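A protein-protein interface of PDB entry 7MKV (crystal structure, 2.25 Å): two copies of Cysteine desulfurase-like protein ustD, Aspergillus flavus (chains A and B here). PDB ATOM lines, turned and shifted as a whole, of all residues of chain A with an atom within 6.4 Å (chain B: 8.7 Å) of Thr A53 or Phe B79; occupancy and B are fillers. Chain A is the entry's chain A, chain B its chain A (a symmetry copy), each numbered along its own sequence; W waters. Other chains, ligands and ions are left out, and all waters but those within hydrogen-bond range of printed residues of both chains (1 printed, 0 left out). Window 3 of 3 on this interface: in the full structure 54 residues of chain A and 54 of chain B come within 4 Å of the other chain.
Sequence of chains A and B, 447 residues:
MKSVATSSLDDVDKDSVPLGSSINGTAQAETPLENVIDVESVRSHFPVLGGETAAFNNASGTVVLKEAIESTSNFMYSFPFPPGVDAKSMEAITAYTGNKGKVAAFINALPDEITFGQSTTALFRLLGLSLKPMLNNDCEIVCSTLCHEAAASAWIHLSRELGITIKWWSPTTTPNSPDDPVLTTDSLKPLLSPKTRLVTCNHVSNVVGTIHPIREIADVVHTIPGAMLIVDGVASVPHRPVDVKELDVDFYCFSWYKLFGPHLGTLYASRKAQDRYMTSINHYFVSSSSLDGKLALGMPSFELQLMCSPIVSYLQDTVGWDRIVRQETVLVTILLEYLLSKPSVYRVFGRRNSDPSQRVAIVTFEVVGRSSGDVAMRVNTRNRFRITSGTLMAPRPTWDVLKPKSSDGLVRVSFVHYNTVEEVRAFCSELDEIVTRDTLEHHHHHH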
ATOM      1  N   VAL A  48      34.204  22.735  -2.626  1.00  0.00           N
ATOM      2  CA  VAL A  48      33.333  22.372  -3.787  1.00  0.00           C
ATOM      3  C   VAL A  48      33.753  23.171  -5.031  1.00  0.00           C
ATOM      4  O   VAL A  48      33.326  22.788  -6.139  1.00  0.00           O
ATOM      5  CB  VAL A  48      31.838  22.575  -3.467  1.00  0.00           C
ATOM      6  CG1 VAL A  48      31.426  24.037  -3.541  1.00  0.00           C
ATOM      7  CG2 VAL A  48      30.948  21.729  -4.367  1.00  0.00           C
ATOM      8  N   LEU A  49      34.561  24.225  -4.866  1.00  0.00           N
ATOM      9  CA  LEU A  49      35.014  25.118  -5.973  1.00  0.00           C
ATOM     10  C   LEU A  49      35.994  24.393  -6.909  1.00  0.00           C
ATOM     11  O   LEU A  49      36.321  24.977  -7.953  1.00  0.00           O
ATOM     12  CB  LEU A  49      35.648  26.383  -5.383  1.00  0.00           C
ATOM     13  CG  LEU A  49      34.685  27.341  -4.682  1.00  0.00           C
ATOM     14  CD1 LEU A  49      35.415  28.576  -4.179  1.00  0.00           C
ATOM     15  CD2 LEU A  49      33.544  27.748  -5.602  1.00  0.00           C
ATOM     16  N   GLY A  50      36.430  23.175  -6.572  1.00  0.00           N
ATOM     17  CA  GLY A  50      37.353  22.368  -7.399  1.00  0.00           C
ATOM     18  C   GLY A  50      36.680  21.710  -8.600  1.00  0.00           C
ATOM     19  O   GLY A  50      37.419  21.253  -9.497  1.00  0.00           O
ATOM     20  N   GLY A  51      35.342  21.659  -8.632  1.00  0.00           N
ATOM     21  CA  GLY A  51      34.555  20.867  -9.601  1.00  0.00           C
ATOM     22  C   GLY A  51      34.447  21.521 -10.971  1.00  0.00           C
ATOM     23  O   GLY A  51      35.246  22.433 -11.263  1.00  0.00           O
ATOM     24  N   GLU A  52      33.484  21.054 -11.777  1.00  0.00           N
ATOM     25  CA  GLU A  52      33.244  21.465 -13.189  1.00  0.00           C
ATOM     26  C   GLU A  52      32.673  22.887 -13.241  1.00  0.00           C
ATOM     27  O   GLU A  52      33.141  23.677 -14.083  1.00  0.00           O
ATOM     28  CB  GLU A  52      32.268  20.495 -13.864  1.00  0.00           C
ATOM     29  CG  GLU A  52      31.942  20.846 -15.308  1.00  0.00           C
ATOM     30  CD  GLU A  52      30.815  20.033 -15.926  1.00  0.00           C
ATOM     31  OE1 GLU A  52      30.423  19.006 -15.328  1.00  0.00           O
ATOM     32  OE2 GLU A  52      30.328  20.431 -17.005  1.00  0.00           O
ATOM     33  N   THR A  53      31.684  23.182 -12.394  1.00  0.00           N
ATOM     34  CA  THR A  53      30.876  24.430 -12.430  1.00  0.00           C
ATOM     35  C   THR A  53      31.582  25.529 -11.625  1.00  0.00           C
ATOM     36  O   THR A  53      31.977  25.262 -10.474  1.00  0.00           O
ATOM     37  CB  THR A  53      29.453  24.172 -11.918  1.00  0.00           C
ATOM     38  OG1 THR A  53      28.982  22.956 -12.502  1.00  0.00           O
ATOM     39  CG2 THR A  53      28.495  25.296 -12.244  1.00  0.00           C
ATOM     40  N   ALA A  54      31.729  26.716 -12.220  1.00  0.00           N
ATOM     41  CA  ALA A  54      32.196  27.956 -11.557  1.00  0.00           C
ATOM     42  C   ALA A  54      30.990  28.689 -10.960  1.00  0.00           C
ATOM     43  O   ALA A  54      29.944  28.748 -11.637  1.00  0.00           O
ATOM     44  CB  ALA A  54      32.930  28.826 -12.545  1.00  0.00           C
ATOM     45  N   ALA A  55      31.141  29.228  -9.746  1.00  0.00           N
ATOM     46  CA  ALA A  55      30.069  29.878  -8.953  1.00  0.00           C
ATOM     47  C   ALA A  55      29.985  31.369  -9.302  1.00  0.00           C
ATOM     48  O   ALA A  55      30.753  32.148  -8.704  1.00  0.00           O
ATOM     49  CB  ALA A  55      30.329  29.674  -7.479  1.00  0.00           C
ATOM     50  N   PHE A  56      29.074  31.741 -10.212  1.00  0.00           N
ATOM     51  CA  PHE A  56      28.890  33.118 -10.753  1.00  0.00           C
ATOM     52  C   PHE A  56      27.478  33.632 -10.441  1.00  0.00           C
ATOM     53  O   PHE A  56      26.989  34.517 -11.179  1.00  0.00           O
ATOM     54  CB  PHE A  56      29.156  33.132 -12.263  1.00  0.00           C
ATOM     55  CG  PHE A  56      30.596  33.308 -12.690  1.00  0.00           C
ATOM     56  CD1 PHE A  56      31.647  33.143 -11.800  1.00  0.00           C
ATOM     57  CD2 PHE A  56      30.897  33.605 -14.011  1.00  0.00           C
ATOM     58  CE1 PHE A  56      32.960  33.298 -12.217  1.00  0.00           C
ATOM     59  CE2 PHE A  56      32.210  33.758 -14.426  1.00  0.00           C
ATOM     60  CZ  PHE A  56      33.240  33.608 -13.528  1.00  0.00           C
ATOM     61  N   VAL A  63      29.159  29.824  -1.474  1.00  0.00           N
ATOM     62  CA  VAL A  63      29.649  28.570  -0.827  1.00  0.00           C
ATOM     63  C   VAL A  63      29.986  28.917   0.626  1.00  0.00           C
ATOM     64  O   VAL A  63      30.513  30.025   0.866  1.00  0.00           O
ATOM     65  CB  VAL A  63      30.860  27.951  -1.549  1.00  0.00           C
ATOM     66  CG1 VAL A  63      31.264  26.632  -0.906  1.00  0.00           C
ATOM     67  CG2 VAL A  63      30.613  27.760  -3.039  1.00  0.00           C
ATOM     68  N   ASN A 380      23.785  27.552 -18.074  1.00  0.00           N
ATOM     69  CA  ASN A 380      23.586  26.681 -16.881  1.00  0.00           C
ATOM     70  C   ASN A 380      23.437  25.215 -17.311  1.00  0.00           C
ATOM     71  O   ASN A 380      23.954  24.346 -16.585  1.00  0.00           O
ATOM     72  CB  ASN A 380      22.402  27.146 -16.029  1.00  0.00           C
ATOM     73  CG  ASN A 380      22.666  28.458 -15.321  1.00  0.00           C
ATOM     74  OD1 ASN A 380      23.813  28.882 -15.196  1.00  0.00           O
ATOM     75  ND2 ASN A 380      21.612  29.112 -14.861  1.00  0.00           N
ATOM     76  N   ARG A 382      24.920  23.803 -19.873  1.00  0.00           N
ATOM     77  CA  ARG A 382      26.336  23.409 -20.123  1.00  0.00           C
ATOM     78  C   ARG A 382      27.036  23.152 -18.783  1.00  0.00           C
ATOM     79  O   ARG A 382      27.855  22.218 -18.716  1.00  0.00           O
ATOM     80  CB  ARG A 382      27.066  24.483 -20.934  1.00  0.00           C
ATOM     81  CG  ARG A 382      26.622  24.561 -22.387  1.00  0.00           C
ATOM     82  CD  ARG A 382      27.450  25.533 -23.207  1.00  0.00           C
ATOM     83  NE  ARG A 382      26.936  25.670 -24.565  1.00  0.00           N
ATOM     84  CZ  ARG A 382      27.507  26.393 -25.526  1.00  0.00           C
ATOM     85  NH1 ARG A 382      28.625  27.059 -25.287  1.00  0.00           N
ATOM     86  NH2 ARG A 382      26.954  26.447 -26.727  1.00  0.00           N
ATOM     87  N   ASN A 383      26.731  23.973 -17.773  1.00  0.00           N
ATOM     88  CA  ASN A 383      27.057  23.735 -16.340  1.00  0.00           C
ATOM     89  C   ASN A 383      28.561  23.920 -16.085  1.00  0.00           C
ATOM     90  O   ASN A 383      29.060  23.357 -15.090  1.00  0.00           O
ATOM     91  CB  ASN A 383      26.575  22.353 -15.885  1.00  0.00           C
ATOM     92  CG  ASN A 383      26.332  22.264 -14.391  1.00  0.00           C
ATOM     93  OD1 ASN A 383      25.916  23.235 -13.762  1.00  0.00           O
ATOM     94  ND2 ASN A 383      26.587  21.100 -13.817  1.00  0.00           N
ATOM     95  N   ARG A 384      29.254  24.682 -16.936  1.00  0.00           N
ATOM     96  CA  ARG A 384      30.646  25.144 -16.689  1.00  0.00           C
ATOM     97  C   ARG A 384      30.583  26.368 -15.768  1.00  0.00           C
ATOM     98  O   ARG A 384      31.499  26.543 -14.941  1.00  0.00           O
ATOM     99  CB  ARG A 384      31.356  25.463 -18.009  1.00  0.00           C
ATOM    100  N   PHE A 385      29.526  27.173 -15.909  1.00  0.00           N
ATOM    101  CA  PHE A 385      29.254  28.389 -15.101  1.00  0.00           C
ATOM    102  C   PHE A 385      27.799  28.375 -14.628  1.00  0.00           C
ATOM    103  O   PHE A 385      26.912  27.929 -15.390  1.00  0.00           O
ATOM    104  CB  PHE A 385      29.563  29.646 -15.918  1.00  0.00           C
ATOM    105  CG  PHE A 385      30.959  29.665 -16.483  1.00  0.00           C
ATOM    106  CD1 PHE A 385      32.017  30.154 -15.734  1.00  0.00           C
ATOM    107  CD2 PHE A 385      31.220  29.154 -17.745  1.00  0.00           C
ATOM    108  CE1 PHE A 385      33.305  30.152 -16.246  1.00  0.00           C
ATOM    109  CE2 PHE A 385      32.509  29.154 -18.257  1.00  0.00           C
ATOM    110  CZ  PHE A 385      33.548  29.653 -17.506  1.00  0.00           C
ATOM    111  N   ARG A 386      27.580  28.840 -13.395  1.00  0.00           N
ATOM    112  CA  ARG A 386      26.243  29.049 -12.786  1.00  0.00           C
ATOM    113  C   ARG A 386      25.958  30.554 -12.764  1.00  0.00           C
ATOM    114  O   ARG A 386      26.648  31.274 -12.015  1.00  0.00           O
ATOM    115  CB  ARG A 386      26.195  28.460 -11.373  1.00  0.00           C
ATOM    116  CG  ARG A 386      24.805  28.434 -10.750  1.00  0.00           C
ATOM    117  CD  ARG A 386      23.858  27.455 -11.425  1.00  0.00           C
ATOM    118  NE  ARG A 386      24.470  26.151 -11.641  1.00  0.00           N
ATOM    119  CZ  ARG A 386      24.626  25.206 -10.716  1.00  0.00           C
ATOM    120  NH1 ARG A 386      25.206  24.061 -11.038  1.00  0.00           N
ATOM    121  NH2 ARG A 386      24.205  25.399  -9.477  1.00  0.00           N
ATOM    122  N   GLU A 423      38.454  31.981 -14.866  1.00  0.00           N
ATOM    123  CA  GLU A 423      37.000  31.667 -14.929  1.00  0.00           C
ATOM    124  C   GLU A 423      36.275  32.737 -15.752  1.00  0.00           C
ATOM    125  O   GLU A 423      35.507  32.358 -16.658  1.00  0.00           O
ATOM    126  CB  GLU A 423      36.392  31.570 -13.529  1.00  0.00           C
ATOM    127  CG  GLU A 423      36.570  30.208 -12.886  1.00  0.00           C
ATOM    128  CD  GLU A 423      35.984  30.095 -11.491  1.00  0.00           C
ATOM    129  OE1 GLU A 423      35.836  31.137 -10.820  1.00  0.00           O
ATOM    130  OE2 GLU A 423      35.687  28.966 -11.070  1.00  0.00           O
ATOM    131  N   SER B  73      26.181  19.234   7.537  1.00  0.00           N
ATOM    132  CA  SER B  73      27.602  19.331   7.109  1.00  0.00           C
ATOM    133  C   SER B  73      27.695  19.065   5.604  1.00  0.00           C
ATOM    134  O   SER B  73      28.249  19.918   4.890  1.00  0.00           O
ATOM    135  CB  SER B  73      28.486  18.383   7.875  1.00  0.00           C
ATOM    136  OG  SER B  73      28.633  18.809   9.221  1.00  0.00           O
ATOM    137  N   ASN B  74      27.141  17.935   5.157  1.00  0.00           N
ATOM    138  CA  ASN B  74      27.188  17.466   3.745  1.00  0.00           C
ATOM    139  C   ASN B  74      26.522  18.499   2.830  1.00  0.00           C
ATOM    140  O   ASN B  74      27.089  18.782   1.759  1.00  0.00           O
ATOM    141  CB  ASN B  74      26.538  16.091   3.581  1.00  0.00           C
ATOM    142  CG  ASN B  74      27.369  14.976   4.185  1.00  0.00           C
ATOM    143  OD1 ASN B  74      28.485  15.206   4.653  1.00  0.00           O
ATOM    144  ND2 ASN B  74      26.836  13.765   4.178  1.00  0.00           N
ATOM    145  N   PHE B  75      25.371  19.041   3.236  1.00  0.00           N
ATOM    146  CA  PHE B  75      24.629  20.075   2.469  1.00  0.00           C
ATOM    147  C   PHE B  75      25.472  21.355   2.367  1.00  0.00           C
ATOM    148  O   PHE B  75      25.570  21.921   1.261  1.00  0.00           O
ATOM    149  CB  PHE B  75      23.269  20.377   3.103  1.00  0.00           C
ATOM    150  CG  PHE B  75      22.530  21.501   2.423  1.00  0.00           C
ATOM    151  CD1 PHE B  75      21.803  21.271   1.263  1.00  0.00           C
ATOM    152  CD2 PHE B  75      22.595  22.797   2.915  1.00  0.00           C
ATOM    153  CE1 PHE B  75      21.138  22.307   0.627  1.00  0.00           C
ATOM    154  CE2 PHE B  75      21.929  23.832   2.276  1.00  0.00           C
ATOM    155  CZ  PHE B  75      21.204  23.585   1.133  1.00  0.00           C
ATOM    156  N   MET B  76      26.057  21.798   3.484  1.00  0.00           N
ATOM    157  CA  MET B  76      26.781  23.095   3.579  1.00  0.00           C
ATOM    158  C   MET B  76      28.147  23.000   2.877  1.00  0.00           C
ATOM    159  O   MET B  76      28.651  24.054   2.462  1.00  0.00           O
ATOM    160  CB  MET B  76      26.946  23.526   5.041  1.00  0.00           C
ATOM    161  CG  MET B  76      25.643  24.015   5.659  1.00  0.00           C
ATOM    162  SD  MET B  76      25.823  24.742   7.313  1.00  0.00           S
ATOM    163  CE  MET B  76      26.293  23.302   8.268  1.00  0.00           C
ATOM    164  N   TYR B  77      28.706  21.791   2.730  1.00  0.00           N
ATOM    165  CA  TYR B  77      29.953  21.516   1.962  1.00  0.00           C
ATOM    166  C   TYR B  77      29.632  21.343   0.470  1.00  0.00           C
ATOM    167  O   TYR B  77      30.574  21.357  -0.343  1.00  0.00           O
ATOM    168  CB  TYR B  77      30.683  20.274   2.491  1.00  0.00           C
ATOM    169  CG  TYR B  77      31.618  20.528   3.647  1.00  0.00           C
ATOM    170  CD1 TYR B  77      32.680  21.412   3.528  1.00  0.00           C
ATOM    171  CD2 TYR B  77      31.457  19.876   4.858  1.00  0.00           C
ATOM    172  CE1 TYR B  77      33.545  21.651   4.583  1.00  0.00           C
ATOM    173  CE2 TYR B  77      32.312  20.104   5.925  1.00  0.00           C
ATOM    174  CZ  TYR B  77      33.361  20.996   5.787  1.00  0.00           C
ATOM    175  OH  TYR B  77      34.209  21.226   6.831  1.00  0.00           O
ATOM    176  N   SER B  78      28.350  21.168   0.130  1.00  0.00           N
ATOM    177  CA  SER B  78      27.846  20.958  -1.254  1.00  0.00           C
ATOM    178  C   SER B  78      27.665  22.311  -1.953  1.00  0.00           C
ATOM    179  O   SER B  78      27.785  23.351  -1.273  1.00  0.00           O
ATOM    180  CB  SER B  78      26.559  20.166  -1.242  1.00  0.00           C
ATOM    181  OG  SER B  78      26.160  19.813  -2.558  1.00  0.00           O
ATOM    182  N   PHE B  79      27.383  22.288  -3.260  1.00  0.00           N
ATOM    183  CA  PHE B  79      27.177  23.495  -4.104  1.00  0.00           C
ATOM    184  C   PHE B  79      25.979  24.271  -3.562  1.00  0.00           C
ATOM    185  O   PHE B  79      24.956  23.672  -3.240  1.00  0.00           O
ATOM    186  CB  PHE B  79      26.990  23.121  -5.578  1.00  0.00           C
ATOM    187  CG  PHE B  79      27.406  24.199  -6.548  1.00  0.00           C
ATOM    188  CD1 PHE B  79      28.729  24.314  -6.953  1.00  0.00           C
ATOM    189  CD2 PHE B  79      26.483  25.105  -7.049  1.00  0.00           C
ATOM    190  CE1 PHE B  79      29.117  25.304  -7.843  1.00  0.00           C
ATOM    191  CE2 PHE B  79      26.873  26.096  -7.939  1.00  0.00           C
ATOM    192  CZ  PHE B  79      28.188  26.193  -8.334  1.00  0.00           C
ATOM    193  N   PRO B  80      26.067  25.616  -3.426  1.00  0.00           N
ATOM    194  CA  PRO B  80      25.024  26.393  -2.753  1.00  0.00           C
ATOM    195  C   PRO B  80      23.689  26.440  -3.511  1.00  0.00           C
ATOM    196  O   PRO B  80      23.694  26.306  -4.724  1.00  0.00           O
ATOM    197  CB  PRO B  80      25.599  27.819  -2.683  1.00  0.00           C
ATOM    198  CG  PRO B  80      27.077  27.654  -2.965  1.00  0.00           C
ATOM    199  CD  PRO B  80      27.171  26.467  -3.897  1.00  0.00           C
ATOM    200  N   PHE B  81      22.589  26.627  -2.775  1.00  0.00           N
ATOM    201  CA  PHE B  81      21.265  27.037  -3.311  1.00  0.00           C
ATOM    202  C   PHE B  81      21.338  28.529  -3.640  1.00  0.00           C
ATOM    203  O   PHE B  81      22.051  29.270  -2.965  1.00  0.00           O
ATOM    204  CB  PHE B  81      20.153  26.690  -2.316  1.00  0.00           C
ATOM    205  CG  PHE B  81      19.646  25.268  -2.388  1.00  0.00           C
ATOM    206  CD1 PHE B  81      20.484  24.218  -2.737  1.00  0.00           C
ATOM    207  CD2 PHE B  81      18.321  24.977  -2.091  1.00  0.00           C
ATOM    208  CE1 PHE B  81      20.007  22.917  -2.800  1.00  0.00           C
ATOM    209  CE2 PHE B  81      17.846  23.674  -2.153  1.00  0.00           C
ATOM    210  CZ  PHE B  81      18.690  22.646  -2.506  1.00  0.00           C
ATOM    211  N   PRO B  82      20.625  29.035  -4.676  1.00  0.00           N
ATOM    212  CA  PRO B  82      19.587  28.282  -5.380  1.00  0.00           C
ATOM    213  C   PRO B  82      20.158  27.338  -6.438  1.00  0.00           C
ATOM    214  O   PRO B  82      21.052  27.712  -7.192  1.00  0.00           O
ATOM    215  CB  PRO B  82      18.743  29.399  -6.015  1.00  0.00           C
ATOM    216  CG  PRO B  82      19.741  30.500  -6.312  1.00  0.00           C
ATOM    217  CD  PRO B  82      20.824  30.370  -5.258  1.00  0.00           C
ATOM    218  N   PRO B  83      19.655  26.086  -6.528  1.00  0.00           N
ATOM    219  CA  PRO B  83      20.251  25.074  -7.402  1.00  0.00           C
ATOM    220  C   PRO B  83      19.946  25.287  -8.895  1.00  0.00           C
ATOM    221  O   PRO B  83      18.975  25.954  -9.209  1.00  0.00           O
ATOM    222  CB  PRO B  83      19.624  23.769  -6.889  1.00  0.00           C
ATOM    223  CG  PRO B  83      18.269  24.190  -6.353  1.00  0.00           C
ATOM    224  CD  PRO B  83      18.478  25.586  -5.802  1.00  0.00           C
ATOM    225  N   GLY B  84      20.780  24.708  -9.765  1.00  0.00           N
ATOM    226  CA  GLY B  84      20.685  24.823 -11.234  1.00  0.00           C
ATOM    227  C   GLY B  84      19.697  23.831 -11.830  1.00  0.00           C
ATOM    228  O   GLY B  84      18.810  23.356 -11.089  1.00  0.00           O
ATOM    229  N   ASP B  86      21.033  21.266 -13.929  1.00  0.00           N
ATOM    230  CA  ASP B  86      21.910  20.091 -14.196  1.00  0.00           C
ATOM    231  C   ASP B  86      21.456  18.899 -13.343  1.00  0.00           C
ATOM    232  O   ASP B  86      20.704  19.112 -12.372  1.00  0.00           O
ATOM    233  CB  ASP B  86      23.385  20.406 -13.933  1.00  0.00           C
ATOM    234  CG  ASP B  86      23.676  20.863 -12.513  1.00  0.00           C
ATOM    235  OD1 ASP B  86      23.234  21.974 -12.160  1.00  0.00           O
ATOM    236  OD2 ASP B  86      24.335  20.102 -11.776  1.00  0.00           O
ATOM    237  N   LYS B  88      23.026  16.871 -11.180  1.00  0.00           N
ATOM    238  CA  LYS B  88      23.492  16.888  -9.765  1.00  0.00           C
ATOM    239  C   LYS B  88      22.666  17.897  -8.955  1.00  0.00           C
ATOM    240  O   LYS B  88      22.397  17.617  -7.770  1.00  0.00           O
ATOM    241  CB  LYS B  88      24.987  17.217  -9.682  1.00  0.00           C
ATOM    242  CG  LYS B  88      25.641  16.860  -8.353  1.00  0.00           C
ATOM    243  CD  LYS B  88      27.091  17.283  -8.241  1.00  0.00           C
ATOM    244  CE  LYS B  88      27.844  16.536  -7.158  1.00  0.00           C
ATOM    245  NZ  LYS B  88      27.135  16.579  -5.856  1.00  0.00           N
ATOM    246  N   SER B  89      22.291  19.028  -9.565  1.00  0.00           N
ATOM    247  CA  SER B  89      21.427  20.075  -8.958  1.00  0.00           C
ATOM    248  C   SER B  89      20.014  19.523  -8.734  1.00  0.00           C
ATOM    249  O   SER B  89      19.433  19.814  -7.675  1.00  0.00           O
ATOM    250  CB  SER B  89      21.402  21.331  -9.798  1.00  0.00           C
ATOM    251  OG  SER B  89      22.654  21.999  -9.745  1.00  0.00           O
ATOM    252  N   ALA B  92      19.881  17.348  -5.734  1.00  0.00           N
ATOM    253  CA  ALA B  92      19.859  18.218  -4.533  1.00  0.00           C
ATOM    254  C   ALA B  92      18.439  18.750  -4.298  1.00  0.00           C
ATOM    255  O   ALA B  92      18.058  18.890  -3.120  1.00  0.00           O
ATOM    256  CB  ALA B  92      20.858  19.341  -4.682  1.00  0.00           C
HETATM  257  O   HOH W   1      32.283  23.370  -0.178  1.00  0.00           O
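The side-chain carboxylate (OD1) of Asp B86 is in salt-bridge range of the guanidinium group (NH1) of Arg A386.
ND2 of Asn A383 lies close to OD2 of Asp B86 (3.2 Å).
NH1 of Arg A386 sits at hydrogen-bond distance from OD1 of Asn A383 (2.9 Å).
The backbone NH of Phe A56 sits close to the backbone carbonyl oxygen of Arg A386.
OG of Ser B89 is in hydrogen-bond range of N of Gly B84 (3.3 Å).
The backbone NH (N) of Arg A386 lies within hydrogen-bond range of the backbone carbonyl oxygen (O) of Ala A54, 2.9 Å away.
OD1 of Asp B86 lies within hydrogen-bond range of OG of Ser B89 (2.5 Å).
The side-chain hydroxyl of Thr A53 lies within hydrogen-bond range of the backbone carbonyl oxygen of Asn A383 (2.6 Å).
CB of Val A48 touches O of Tyr B77 (3.6 Å).
Phe B79 touches Val A48 (N to CG2, 3.8 Å).
CE1 of Phe B79 touches O of Thr A53, at 3.9 Å.
CG of Pro B80 touches N of Val A63, 3.4 Å away.
NH2 of Arg A386 touches CE2 of Phe B79, at 3.2 Å.
Gly B84 touches Arg A386.
Arg A386 touches Ser B89.
Thr A53 touches one residue of chain B.
Of chain A, only Val A48, Thr A53 and Arg A386 come within 4 Å of Phe B79.
No residue of chain B comes within 4 Å of Ala A54.
Printed residues of chain A within 4 Å of Asp B86: Asn A383 (3.2 Å) and Arg A386 (3.1 Å).
Printed residues of chain A within 4 Å of Pro B80: Val A63.
Of the printed residues of chain A, Ser B89 touches Arg A386.
Of the printed residues of chain B, Val A63 touches Pro B80.
Phe B75 touches none of the printed residues of chain A.
The nearest residue of chain A that does not touch Phe B79 is Ala A55 (4.2 Å).
Of the 17 printed residues of chain A, 5 touch a printed residue of chain B.
Hydrophobic or aromatic side chains of chain B within 4 Å of the printed part of chain A: Phe B79 and Pro B80.
Among the printed residues, 9 pairs touch across the chains.
Among the printed residues, Asp or Glu carboxylates within 4 Å of a Lys or Arg side-chain nitrogen of the other chain: Arg A386 with Asp B86 (3.1 Å).
No position is printed for both chains.
Water W1 bridges the backbone carbonyl oxygen of Tyr B77 (2.6 Å) and the backbone NH of Val A48 (3.2 Å).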
